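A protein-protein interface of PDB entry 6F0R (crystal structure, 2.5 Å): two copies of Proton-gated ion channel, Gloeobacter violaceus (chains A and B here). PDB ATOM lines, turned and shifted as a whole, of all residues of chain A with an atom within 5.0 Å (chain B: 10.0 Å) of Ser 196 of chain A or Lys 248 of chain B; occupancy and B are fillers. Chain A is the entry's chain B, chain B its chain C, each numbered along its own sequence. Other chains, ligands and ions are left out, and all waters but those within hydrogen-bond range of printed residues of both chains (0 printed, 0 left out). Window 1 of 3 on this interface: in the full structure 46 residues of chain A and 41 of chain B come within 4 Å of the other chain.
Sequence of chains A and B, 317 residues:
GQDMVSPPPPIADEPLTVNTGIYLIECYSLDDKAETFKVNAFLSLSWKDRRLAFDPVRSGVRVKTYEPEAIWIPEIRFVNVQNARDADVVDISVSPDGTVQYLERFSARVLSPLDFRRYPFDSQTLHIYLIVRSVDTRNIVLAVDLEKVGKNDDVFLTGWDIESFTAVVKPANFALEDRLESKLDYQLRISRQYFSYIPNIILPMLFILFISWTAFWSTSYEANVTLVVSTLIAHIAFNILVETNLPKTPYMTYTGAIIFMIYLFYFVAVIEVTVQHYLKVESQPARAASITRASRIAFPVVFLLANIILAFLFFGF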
ATOM      1  N   TYR A 119      -0.983  30.034  -8.601  1.00  0.00           N
ATOM      2  CA  TYR A 119      -2.055  29.641  -9.520  1.00  0.00           C
ATOM      3  C   TYR A 119      -1.491  29.139 -10.876  1.00  0.00           C
ATOM      4  O   TYR A 119      -0.590  29.779 -11.429  1.00  0.00           O
ATOM      5  CB  TYR A 119      -3.016  30.824  -9.728  1.00  0.00           C
ATOM      6  CG  TYR A 119      -4.170  30.550 -10.657  1.00  0.00           C
ATOM      7  CD1 TYR A 119      -4.079  30.832 -12.021  1.00  0.00           C
ATOM      8  CD2 TYR A 119      -5.370  30.046 -10.176  1.00  0.00           C
ATOM      9  CE1 TYR A 119      -5.150  30.592 -12.882  1.00  0.00           C
ATOM     10  CE2 TYR A 119      -6.452  29.820 -11.022  1.00  0.00           C
ATOM     11  CZ  TYR A 119      -6.336  30.083 -12.377  1.00  0.00           C
ATOM     12  OH  TYR A 119      -7.407  29.844 -13.207  1.00  0.00           O
ATOM     13  N   GLY A 159     -13.412  21.150  -9.371  1.00  0.00           N
ATOM     14  CA  GLY A 159     -12.104  21.706  -9.693  1.00  0.00           C
ATOM     15  C   GLY A 159     -11.074  21.718  -8.580  1.00  0.00           C
ATOM     16  O   GLY A 159     -10.007  22.324  -8.717  1.00  0.00           O
ATOM     17  N   GLN A 193      -7.033  21.251  -8.691  1.00  0.00           N
ATOM     18  CA  GLN A 193      -6.873  20.253  -9.746  1.00  0.00           C
ATOM     19  C   GLN A 193      -6.363  21.024 -10.970  1.00  0.00           C
ATOM     20  O   GLN A 193      -7.154  21.511 -11.809  1.00  0.00           O
ATOM     21  CB  GLN A 193      -8.197  19.535 -10.036  1.00  0.00           C
ATOM     22  CG  GLN A 193      -8.627  18.613  -8.924  1.00  0.00           C
ATOM     23  CD  GLN A 193      -9.952  17.943  -9.151  1.00  0.00           C
ATOM     24  OE1 GLN A 193     -10.904  18.503  -9.720  1.00  0.00           O
ATOM     25  NE2 GLN A 193     -10.060  16.749  -8.611  1.00  0.00           N
ATOM     26  N   TYR A 194      -5.020  21.178 -11.022  1.00  0.00           N
ATOM     27  CA  TYR A 194      -4.288  21.930 -12.056  1.00  0.00           C
ATOM     28  C   TYR A 194      -4.274  21.283 -13.461  1.00  0.00           C
ATOM     29  O   TYR A 194      -3.879  21.951 -14.416  1.00  0.00           O
ATOM     30  CB  TYR A 194      -2.850  22.224 -11.593  1.00  0.00           C
ATOM     31  CG  TYR A 194      -2.006  20.989 -11.352  1.00  0.00           C
ATOM     32  CD1 TYR A 194      -1.458  20.272 -12.418  1.00  0.00           C
ATOM     33  CD2 TYR A 194      -1.702  20.571 -10.064  1.00  0.00           C
ATOM     34  CE1 TYR A 194      -0.692  19.129 -12.201  1.00  0.00           C
ATOM     35  CE2 TYR A 194      -0.928  19.435  -9.837  1.00  0.00           C
ATOM     36  CZ  TYR A 194      -0.430  18.716 -10.910  1.00  0.00           C
ATOM     37  OH  TYR A 194       0.313  17.592 -10.683  1.00  0.00           O
ATOM     38  N   PHE A 195      -4.656  19.995 -13.568  1.00  0.00           N
ATOM     39  CA  PHE A 195      -4.672  19.184 -14.784  1.00  0.00           C
ATOM     40  C   PHE A 195      -5.149  19.914 -16.044  1.00  0.00           C
ATOM     41  O   PHE A 195      -4.353  20.064 -16.960  1.00  0.00           O
ATOM     42  CB  PHE A 195      -5.475  17.881 -14.582  1.00  0.00           C
ATOM     43  CG  PHE A 195      -5.507  17.001 -15.813  1.00  0.00           C
ATOM     44  CD1 PHE A 195      -6.419  17.235 -16.838  1.00  0.00           C
ATOM     45  CD2 PHE A 195      -4.613  15.958 -15.960  1.00  0.00           C
ATOM     46  CE1 PHE A 195      -6.403  16.466 -17.998  1.00  0.00           C
ATOM     47  CE2 PHE A 195      -4.592  15.194 -17.135  1.00  0.00           C
ATOM     48  CZ  PHE A 195      -5.499  15.443 -18.131  1.00  0.00           C
ATOM     49  N   SER A 196      -6.432  20.313 -16.122  1.00  0.00           N
ATOM     50  CA  SER A 196      -7.055  20.953 -17.287  1.00  0.00           C
ATOM     51  C   SER A 196      -6.322  22.177 -17.788  1.00  0.00           C
ATOM     52  O   SER A 196      -6.310  22.405 -19.001  1.00  0.00           O
ATOM     53  CB  SER A 196      -8.527  21.268 -17.052  1.00  0.00           C
ATOM     54  OG  SER A 196      -8.694  22.085 -15.906  1.00  0.00           O
ATOM     55  N   TYR A 197      -5.647  22.920 -16.902  1.00  0.00           N
ATOM     56  CA  TYR A 197      -4.849  24.102 -17.284  1.00  0.00           C
ATOM     57  C   TYR A 197      -3.749  23.793 -18.274  1.00  0.00           C
ATOM     58  O   TYR A 197      -3.391  24.659 -19.064  1.00  0.00           O
ATOM     59  CB  TYR A 197      -4.261  24.764 -16.032  1.00  0.00           C
ATOM     60  CG  TYR A 197      -5.338  25.345 -15.149  1.00  0.00           C
ATOM     61  CD1 TYR A 197      -5.940  24.580 -14.151  1.00  0.00           C
ATOM     62  CD2 TYR A 197      -5.807  26.635 -15.353  1.00  0.00           C
ATOM     63  CE1 TYR A 197      -6.968  25.098 -13.359  1.00  0.00           C
ATOM     64  CE2 TYR A 197      -6.824  27.169 -14.558  1.00  0.00           C
ATOM     65  CZ  TYR A 197      -7.409  26.397 -13.568  1.00  0.00           C
ATOM     66  OH  TYR A 197      -8.436  26.952 -12.828  1.00  0.00           O
ATOM     67  N   ILE A 198      -3.228  22.559 -18.244  1.00  0.00           N
ATOM     68  CA  ILE A 198      -2.162  22.092 -19.132  1.00  0.00           C
ATOM     69  C   ILE A 198      -2.665  21.937 -20.582  1.00  0.00           C
ATOM     70  O   ILE A 198      -2.139  22.672 -21.425  1.00  0.00           O
ATOM     71  CB  ILE A 198      -1.447  20.826 -18.581  1.00  0.00           C
ATOM     72  CG1 ILE A 198      -0.992  21.038 -17.112  1.00  0.00           C
ATOM     73  CG2 ILE A 198      -0.291  20.397 -19.522  1.00  0.00           C
ATOM     74  CD1 ILE A 198      -0.583  19.804 -16.396  1.00  0.00           C
ATOM     75  N   PRO A 199      -3.654  21.058 -20.939  1.00  0.00           N
ATOM     76  CA  PRO A 199      -4.072  20.988 -22.357  1.00  0.00           C
ATOM     77  C   PRO A 199      -4.878  22.192 -22.885  1.00  0.00           C
ATOM     78  O   PRO A 199      -5.001  22.365 -24.106  1.00  0.00           O
ATOM     79  CB  PRO A 199      -4.879  19.691 -22.419  1.00  0.00           C
ATOM     80  CG  PRO A 199      -5.433  19.525 -21.050  1.00  0.00           C
ATOM     81  CD  PRO A 199      -4.392  20.065 -20.123  1.00  0.00           C
ATOM     82  N   ASN A 200      -5.420  23.023 -21.987  1.00  0.00           N
ATOM     83  CA  ASN A 200      -6.287  24.138 -22.377  1.00  0.00           C
ATOM     84  C   ASN A 200      -5.635  25.510 -22.464  1.00  0.00           C
ATOM     85  O   ASN A 200      -6.091  26.326 -23.277  1.00  0.00           O
ATOM     86  CB  ASN A 200      -7.513  24.213 -21.472  1.00  0.00           C
ATOM     87  CG  ASN A 200      -8.425  23.027 -21.650  1.00  0.00           C
ATOM     88  OD1 ASN A 200      -8.973  22.761 -22.737  1.00  0.00           O
ATOM     89  ND2 ASN A 200      -8.590  22.283 -20.592  1.00  0.00           N
ATOM     90  N   ILE A 201      -4.640  25.796 -21.605  1.00  0.00           N
ATOM     91  CA  ILE A 201      -3.976  27.100 -21.575  1.00  0.00           C
ATOM     92  C   ILE A 201      -2.453  26.976 -21.750  1.00  0.00           C
ATOM     93  O   ILE A 201      -1.922  27.583 -22.669  1.00  0.00           O
ATOM     94  CB  ILE A 201      -4.377  27.951 -20.304  1.00  0.00           C
ATOM     95  CG1 ILE A 201      -5.829  28.440 -20.367  1.00  0.00           C
ATOM     96  CG2 ILE A 201      -3.483  29.179 -20.190  1.00  0.00           C
ATOM     97  CD1 ILE A 201      -6.653  27.829 -19.522  1.00  0.00           C
ATOM     98  N   ASN A 245     -10.804  34.630 -15.456  1.00  0.00           N
ATOM     99  CA  ASN A 245     -11.033  33.532 -14.491  1.00  0.00           C
ATOM    100  C   ASN A 245     -10.552  33.875 -13.071  1.00  0.00           C
ATOM    101  O   ASN A 245     -10.822  33.115 -12.128  1.00  0.00           O
ATOM    102  CB  ASN A 245     -10.275  32.231 -14.930  1.00  0.00           C
ATOM    103  CG  ASN A 245     -10.298  31.758 -16.389  1.00  0.00           C
ATOM    104  OD1 ASN A 245      -9.386  31.027 -16.829  1.00  0.00           O
ATOM    105  ND2 ASN A 245     -11.343  32.089 -17.157  1.00  0.00           N
ATOM    106  N   ASP B  32     -24.165  22.286 -17.241  1.00  0.00           N
ATOM    107  CA  ASP B  32     -22.976  21.444 -17.347  1.00  0.00           C
ATOM    108  C   ASP B  32     -21.796  21.984 -16.518  1.00  0.00           C
ATOM    109  O   ASP B  32     -21.123  21.210 -15.843  1.00  0.00           O
ATOM    110  CB  ASP B  32     -22.575  21.258 -18.830  1.00  0.00           C
ATOM    111  CG  ASP B  32     -23.636  20.588 -19.677  1.00  0.00           C
ATOM    112  OD1 ASP B  32     -24.474  21.316 -20.266  1.00  0.00           O
ATOM    113  OD2 ASP B  32     -23.652  19.339 -19.729  1.00  0.00           O
ATOM    114  N   LYS B  33     -21.568  23.305 -16.557  1.00  0.00           N
ATOM    115  CA  LYS B  33     -20.477  23.989 -15.862  1.00  0.00           C
ATOM    116  C   LYS B  33     -20.607  23.890 -14.345  1.00  0.00           C
ATOM    117  O   LYS B  33     -19.633  23.545 -13.660  1.00  0.00           O
ATOM    118  CB  LYS B  33     -20.415  25.451 -16.321  1.00  0.00           C
ATOM    119  CG  LYS B  33     -19.017  25.890 -16.659  1.00  0.00           C
ATOM    120  CD  LYS B  33     -18.968  27.296 -17.231  1.00  0.00           C
ATOM    121  CE  LYS B  33     -17.560  27.877 -17.202  1.00  0.00           C
ATOM    122  NZ  LYS B  33     -16.560  27.076 -17.980  1.00  0.00           N
ATOM    123  N   ALA B  34     -21.828  24.153 -13.821  1.00  0.00           N
ATOM    124  CA  ALA B  34     -22.143  24.084 -12.399  1.00  0.00           C
ATOM    125  C   ALA B  34     -22.407  22.657 -11.914  1.00  0.00           C
ATOM    126  O   ALA B  34     -22.308  22.397 -10.714  1.00  0.00           O
ATOM    127  CB  ALA B  34     -23.344  24.955 -12.100  1.00  0.00           C
ATOM    128  N   GLU B  35     -22.758  21.746 -12.841  1.00  0.00           N
ATOM    129  CA  GLU B  35     -23.121  20.343 -12.608  1.00  0.00           C
ATOM    130  C   GLU B  35     -24.358  20.249 -11.709  1.00  0.00           C
ATOM    131  O   GLU B  35     -24.416  19.493 -10.734  1.00  0.00           O
ATOM    132  CB  GLU B  35     -21.939  19.506 -12.130  1.00  0.00           C
ATOM    133  CG  GLU B  35     -21.019  19.107 -13.271  1.00  0.00           C
ATOM    134  CD  GLU B  35     -19.701  18.568 -12.785  1.00  0.00           C
ATOM    135  OE1 GLU B  35     -18.782  19.388 -12.565  1.00  0.00           O
ATOM    136  OE2 GLU B  35     -19.604  17.340 -12.559  1.00  0.00           O
ATOM    137  N   LEU B 114     -21.433  15.219 -13.245  1.00  0.00           N
ATOM    138  CA  LEU B 114     -21.448  14.680 -14.590  1.00  0.00           C
ATOM    139  C   LEU B 114     -20.084  14.167 -14.970  1.00  0.00           C
ATOM    140  O   LEU B 114     -19.087  14.682 -14.468  1.00  0.00           O
ATOM    141  CB  LEU B 114     -21.978  15.743 -15.573  1.00  0.00           C
ATOM    142  CG  LEU B 114     -23.261  16.477 -15.120  1.00  0.00           C
ATOM    143  CD1 LEU B 114     -23.477  17.741 -15.876  1.00  0.00           C
ATOM    144  CD2 LEU B 114     -24.455  15.608 -15.273  1.00  0.00           C
ATOM    145  N   PHE B 116     -17.837  13.908 -18.051  1.00  0.00           N
ATOM    146  CA  PHE B 116     -17.682  14.468 -19.391  1.00  0.00           C
ATOM    147  C   PHE B 116     -16.720  13.720 -20.306  1.00  0.00           C
ATOM    148  O   PHE B 116     -16.552  14.153 -21.450  1.00  0.00           O
ATOM    149  CB  PHE B 116     -17.299  15.951 -19.323  1.00  0.00           C
ATOM    150  CG  PHE B 116     -18.302  16.819 -18.617  1.00  0.00           C
ATOM    151  CD1 PHE B 116     -19.418  17.308 -19.290  1.00  0.00           C
ATOM    152  CD2 PHE B 116     -18.150  17.131 -17.268  1.00  0.00           C
ATOM    153  CE1 PHE B 116     -20.365  18.087 -18.619  1.00  0.00           C
ATOM    154  CE2 PHE B 116     -19.107  17.908 -16.605  1.00  0.00           C
ATOM    155  CZ  PHE B 116     -20.193  18.394 -17.286  1.00  0.00           C
ATOM    156  N   ASN B 239     -11.595  26.184 -29.481  1.00  0.00           N
ATOM    157  CA  ASN B 239     -11.127  25.620 -28.211  1.00  0.00           C
ATOM    158  C   ASN B 239     -11.659  26.474 -27.040  1.00  0.00           C
ATOM    159  O   ASN B 239     -12.183  25.918 -26.071  1.00  0.00           O
ATOM    160  CB  ASN B 239      -9.600  25.539 -28.166  1.00  0.00           C
ATOM    161  CG  ASN B 239      -9.018  24.901 -26.917  1.00  0.00           C
ATOM    162  OD1 ASN B 239      -9.710  24.540 -25.948  1.00  0.00           O
ATOM    163  ND2 ASN B 239      -7.720  24.691 -26.912  1.00  0.00           N
ATOM    164  N   ILE B 240     -11.575  27.816 -27.155  1.00  0.00           N
ATOM    165  CA  ILE B 240     -12.080  28.700 -26.099  1.00  0.00           C
ATOM    166  C   ILE B 240     -13.574  28.547 -25.964  1.00  0.00           C
ATOM    167  O   ILE B 240     -14.054  28.484 -24.848  1.00  0.00           O
ATOM    168  CB  ILE B 240     -11.627  30.175 -26.285  1.00  0.00           C
ATOM    169  CG1 ILE B 240     -10.071  30.290 -26.115  1.00  0.00           C
ATOM    170  CG2 ILE B 240     -12.418  31.130 -25.329  1.00  0.00           C
ATOM    171  CD1 ILE B 240      -9.420  31.595 -26.550  1.00  0.00           C
ATOM    172  N   VAL B 242     -15.545  25.887 -26.731  1.00  0.00           N
ATOM    173  CA  VAL B 242     -15.805  24.582 -26.120  1.00  0.00           C
ATOM    174  C   VAL B 242     -15.523  24.588 -24.611  1.00  0.00           C
ATOM    175  O   VAL B 242     -16.376  24.136 -23.846  1.00  0.00           O
ATOM    176  CB  VAL B 242     -15.053  23.451 -26.874  1.00  0.00           C
ATOM    177  CG1 VAL B 242     -15.048  22.142 -26.085  1.00  0.00           C
ATOM    178  CG2 VAL B 242     -15.637  23.246 -28.268  1.00  0.00           C
ATOM    179  N   GLU B 243     -14.373  25.145 -24.178  1.00  0.00           N
ATOM    180  CA  GLU B 243     -13.987  25.124 -22.770  1.00  0.00           C
ATOM    181  C   GLU B 243     -14.844  26.063 -21.904  1.00  0.00           C
ATOM    182  O   GLU B 243     -14.944  25.806 -20.697  1.00  0.00           O
ATOM    183  CB  GLU B 243     -12.468  25.303 -22.567  1.00  0.00           C
ATOM    184  CG  GLU B 243     -11.887  26.686 -22.738  1.00  0.00           C
ATOM    185  CD  GLU B 243     -10.426  26.770 -22.328  1.00  0.00           C
ATOM    186  OE1 GLU B 243      -9.534  26.656 -23.203  1.00  0.00           O
ATOM    187  OE2 GLU B 243     -10.176  26.930 -21.111  1.00  0.00           O
ATOM    188  N   THR B 244     -15.553  27.048 -22.499  1.00  0.00           N
ATOM    189  CA  THR B 244     -16.494  27.910 -21.752  1.00  0.00           C
ATOM    190  C   THR B 244     -17.797  27.170 -21.421  1.00  0.00           C
ATOM    191  O   THR B 244     -18.433  27.526 -20.443  1.00  0.00           O
ATOM    192  CB  THR B 244     -16.831  29.252 -22.480  1.00  0.00           C
ATOM    193  OG1 THR B 244     -17.586  29.026 -23.681  1.00  0.00           O
ATOM    194  CG2 THR B 244     -15.614  30.129 -22.751  1.00  0.00           C
ATOM    195  N   ASN B 245     -18.208  26.165 -22.239  1.00  0.00           N
ATOM    196  CA  ASN B 245     -19.457  25.376 -22.089  1.00  0.00           C
ATOM    197  C   ASN B 245     -19.334  24.251 -21.051  1.00  0.00           C
ATOM    198  O   ASN B 245     -20.353  23.638 -20.696  1.00  0.00           O
ATOM    199  CB  ASN B 245     -19.869  24.695 -23.432  1.00  0.00           C
ATOM    200  CG  ASN B 245     -19.829  25.473 -24.733  1.00  0.00           C
ATOM    201  OD1 ASN B 245     -19.723  24.868 -25.827  1.00  0.00           O
ATOM    202  ND2 ASN B 245     -19.983  26.800 -24.673  1.00  0.00           N
ATOM    203  N   LEU B 246     -18.092  23.926 -20.650  1.00  0.00           N
ATOM    204  CA  LEU B 246     -17.755  22.801 -19.787  1.00  0.00           C
ATOM    205  C   LEU B 246     -16.998  23.229 -18.539  1.00  0.00           C
ATOM    206  O   LEU B 246     -16.229  24.200 -18.590  1.00  0.00           O
ATOM    207  CB  LEU B 246     -16.785  21.882 -20.571  1.00  0.00           C
ATOM    208  CG  LEU B 246     -17.301  21.074 -21.735  1.00  0.00           C
ATOM    209  CD1 LEU B 246     -16.166  20.527 -22.509  1.00  0.00           C
ATOM    210  CD2 LEU B 246     -18.191  19.950 -21.264  1.00  0.00           C
ATOM    211  N   PRO B 247     -17.051  22.437 -17.451  1.00  0.00           N
ATOM    212  CA  PRO B 247     -16.204  22.764 -16.298  1.00  0.00           C
ATOM    213  C   PRO B 247     -14.792  22.181 -16.488  1.00  0.00           C
ATOM    214  O   PRO B 247     -14.576  21.327 -17.357  1.00  0.00           O
ATOM    215  CB  PRO B 247     -16.935  22.094 -15.130  1.00  0.00           C
ATOM    216  CG  PRO B 247     -17.612  20.928 -15.737  1.00  0.00           C
ATOM    217  CD  PRO B 247     -17.858  21.223 -17.195  1.00  0.00           C
ATOM    218  N   LYS B 248     -13.851  22.628 -15.649  1.00  0.00           N
ATOM    219  CA  LYS B 248     -12.468  22.175 -15.626  1.00  0.00           C
ATOM    220  C   LYS B 248     -12.422  20.783 -14.963  1.00  0.00           C
ATOM    221  O   LYS B 248     -12.598  20.671 -13.744  1.00  0.00           O
ATOM    222  CB  LYS B 248     -11.602  23.196 -14.873  1.00  0.00           C
ATOM    223  CG  LYS B 248     -11.419  24.497 -15.639  1.00  0.00           C
ATOM    224  CD  LYS B 248     -11.025  25.635 -14.728  1.00  0.00           C
ATOM    225  CE  LYS B 248     -10.984  26.912 -15.535  1.00  0.00           C
ATOM    226  NZ  LYS B 248     -10.396  28.030 -14.749  1.00  0.00           N
ATOM    227  N   THR B 249     -12.169  19.729 -15.781  1.00  0.00           N
ATOM    228  CA  THR B 249     -12.114  18.312 -15.379  1.00  0.00           C
ATOM    229  C   THR B 249     -10.682  17.803 -15.123  1.00  0.00           C
ATOM    230  O   THR B 249      -9.786  18.145 -15.875  1.00  0.00           O
ATOM    231  CB  THR B 249     -12.855  17.417 -16.393  1.00  0.00           C
ATOM    232  OG1 THR B 249     -12.272  17.591 -17.693  1.00  0.00           O
ATOM    233  CG2 THR B 249     -14.368  17.682 -16.426  1.00  0.00           C
ATOM    234  N   PRO B 250     -10.438  16.959 -14.085  1.00  0.00           N
ATOM    235  CA  PRO B 250      -9.067  16.439 -13.880  1.00  0.00           C
ATOM    236  C   PRO B 250      -8.752  15.234 -14.785  1.00  0.00           C
ATOM    237  O   PRO B 250      -7.925  14.385 -14.452  1.00  0.00           O
ATOM    238  CB  PRO B 250      -9.091  16.047 -12.387  1.00  0.00           C
ATOM    239  CG  PRO B 250     -10.520  15.670 -12.128  1.00  0.00           C
ATOM    240  CD  PRO B 250     -11.384  16.420 -13.073  1.00  0.00           C
ATOM    241  N   TYR B 251      -9.450  15.142 -15.910  1.00  0.00           N
ATOM    242  CA  TYR B 251      -9.348  14.073 -16.899  1.00  0.00           C
ATOM    243  C   TYR B 251      -9.616  14.664 -18.254  1.00  0.00           C
ATOM    244  O   TYR B 251     -10.197  15.747 -18.339  1.00  0.00           O
ATOM    245  CB  TYR B 251     -10.368  12.942 -16.620  1.00  0.00           C
ATOM    246  CG  TYR B 251     -11.817  13.390 -16.529  1.00  0.00           C
ATOM    247  CD1 TYR B 251     -12.572  13.636 -17.682  1.00  0.00           C
ATOM    248  CD2 TYR B 251     -12.451  13.518 -15.292  1.00  0.00           C
ATOM    249  CE1 TYR B 251     -13.903  14.041 -17.602  1.00  0.00           C
ATOM    250  CE2 TYR B 251     -13.783  13.918 -15.204  1.00  0.00           C
ATOM    251  CZ  TYR B 251     -14.509  14.162 -16.358  1.00  0.00           C
ATOM    252  OH  TYR B 251     -15.819  14.559 -16.265  1.00  0.00           O
ATOM    253  N   MET B 252      -9.246  13.948 -19.311  1.00  0.00           N
ATOM    254  CA  MET B 252      -9.489  14.439 -20.663  1.00  0.00           C
ATOM    255  C   MET B 252     -10.865  14.007 -21.129  1.00  0.00           C
ATOM    256  O   MET B 252     -11.277  12.869 -20.870  1.00  0.00           O
ATOM    257  CB  MET B 252      -8.422  13.895 -21.628  1.00  0.00           C
ATOM    258  CG  MET B 252      -7.950  14.910 -22.623  1.00  0.00           C
ATOM    259  SD  MET B 252      -6.746  16.072 -21.927  1.00  0.00           S
ATOM    260  CE  MET B 252      -5.595  14.938 -21.254  1.00  0.00           C
ATOM    261  N   THR B 253     -11.577  14.924 -21.796  1.00  0.00           N
ATOM    262  CA  THR B 253     -12.878  14.678 -22.424  1.00  0.00           C
ATOM    263  C   THR B 253     -12.573  14.324 -23.890  1.00  0.00           C
ATOM    264  O   THR B 253     -11.459  14.599 -24.373  1.00  0.00           O
ATOM    265  CB  THR B 253     -13.828  15.881 -22.272  1.00  0.00           C
ATOM    266  OG1 THR B 253     -13.320  17.008 -22.981  1.00  0.00           O
ATOM    267  CG2 THR B 253     -14.063  16.258 -20.812  1.00  0.00           C
ATOM    268  N   GLY B 256     -12.092  17.415 -25.977  1.00  0.00           N
ATOM    269  CA  GLY B 256     -10.889  18.052 -25.484  1.00  0.00           C
ATOM    270  C   GLY B 256      -9.619  17.438 -26.025  1.00  0.00           C
ATOM    271  O   GLY B 256      -8.653  18.169 -26.279  1.00  0.00           O
ATOM    272  N   PHE B 260      -7.105  19.245 -28.550  1.00  0.00           N
ATOM    273  CA  PHE B 260      -5.680  19.281 -28.208  1.00  0.00           C
ATOM    274  C   PHE B 260      -4.786  18.690 -29.325  1.00  0.00           C
ATOM    275  O   PHE B 260      -3.783  19.299 -29.689  1.00  0.00           O
ATOM    276  CB  PHE B 260      -5.398  18.593 -26.856  1.00  0.00           C
ATOM    277  CG  PHE B 260      -3.942  18.664 -26.500  1.00  0.00           C
ATOM    278  CD1 PHE B 260      -3.356  19.872 -26.138  1.00  0.00           C
ATOM    279  CD2 PHE B 260      -3.127  17.542 -26.607  1.00  0.00           C
ATOM    280  CE1 PHE B 260      -1.984  19.948 -25.866  1.00  0.00           C
ATOM    281  CE2 PHE B 260      -1.748  17.627 -26.372  1.00  0.00           C
ATOM    282  CZ  PHE B 260      -1.190  18.828 -26.002  1.00  0.00           C
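The backbone carbonyl oxygen (O) of Asn 200 of chain A lies close to the side-chain carboxylate (OE1) of Glu 243 of chain B (3.5 Å).
OH of Tyr 197 of chain A sits at hydrogen-bond distance from NZ of Lys 248 of chain B, at 2.9 Å.
The backbone NH (N) of Gln 193 of chain A sits at hydrogen-bond distance from the backbone carbonyl oxygen (O) of Gly 159 of chain A.
OH of Tyr 197 of chain A lies close to OH of Tyr 119 of chain A, 3.1 Å away.
OE1 of Glu 243 of chain B sits close to OD1 of Asn 239 of chain B.
The backbone carbonyl oxygen (O) of Ser 196 of chain A sits at hydrogen-bond distance from the side-chain amide nitrogen (ND2) of Asn 200 of chain A (2.8 Å).
N of Phe 116 of chain B is in hydrogen-bond range of OH of Tyr 251 of chain B (2.8 Å).
The side-chain amino group of Lys 33 of chain B is in hydrogen-bond range of the backbone carbonyl oxygen of Glu 243 of chain B (3.4 Å).
Lys 248 of chain B touches Tyr 119 of chain A (NZ to OH, 3.8 Å).
Gln 193 of chain A touches Pro 250 of chain B.
CD1 of Phe 195 of chain A touches O of Thr 249 of chain B, at 3.6 Å.
Met 252 of chain B touches Phe 195 of chain A.
CB of Ser 196 of chain A touches O of Thr 249 of chain B, 3.6 Å away.
SD of Met 252 of chain B touches CG of Pro 199 of chain A, 3.8 Å away.
O of Pro 199 of chain A touches CD1 of Phe 260 of chain B (3.6 Å).
Asn 239 of chain B touches Asn 200 of chain A (OD1 to OD1, 3.7 Å).
Ile 201 of chain A touches Glu 243 of chain B (CD1 to OE2, 3.97 Å).
Lys 248 of chain B touches Asn 245 of chain A.
Phe 195 of chain A touches just these residues of chain B: Thr 249, Pro 250, Tyr 251 and Met 252.
Ser 196 of chain A touches two residues of chain B.
Tyr 197 of chain A touches one residue of chain B.
Of chain B, only Met 252 and Phe 260 come within 4 Å of Pro 199 of chain A.
Of chain B, only Asn 239 and Glu 243 come within 4 Å of Asn 200 of chain A.
Of the printed residues of chain B, Ile 201 of chain A touches Glu 243 (3.97 Å).
Of the printed residues of chain A, Glu 243 of chain B touches Asn 200 (3.5 Å) and Ile 201 (3.97 Å).
Thr 244 of chain B touches none of the printed residues of chain A.
Of the printed residues of chain A, Thr 249 of chain B touches Phe 195 and Ser 196.
Of the printed residues of chain A, Met 252 of chain B touches Phe 195 and Pro 199.
The nearest residue of chain B that does not touch Ser 196 of chain A is Pro 250 of chain B (5.2 Å).
Of the 22 printed residues of chain B, 8 touch a printed residue of chain A.
Hydrophobic or aromatic side chains of chain B within 4 Å of the printed part of chain A: Pro 250, Met 252 and Phe 260.
Printed residues of chain A that touch a printed residue of chain B: Tyr 119, Gln 193, Phe 195, Ser 196, Tyr 197, Pro 199, Asn 200, Ile 201 and Asn 245.
Hydrophobic or aromatic side chains of chain A that line the printed part of chain B: Tyr 119, Phe 195, Tyr 197, Pro 199 and Ile 201.
Among the printed residues, 15 pairs touch across the chains.
1 position is printed for both chains.
Of the 15 pairs that touch across the chains among the printed residues, none has its exchanged pair printed and touching as well.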
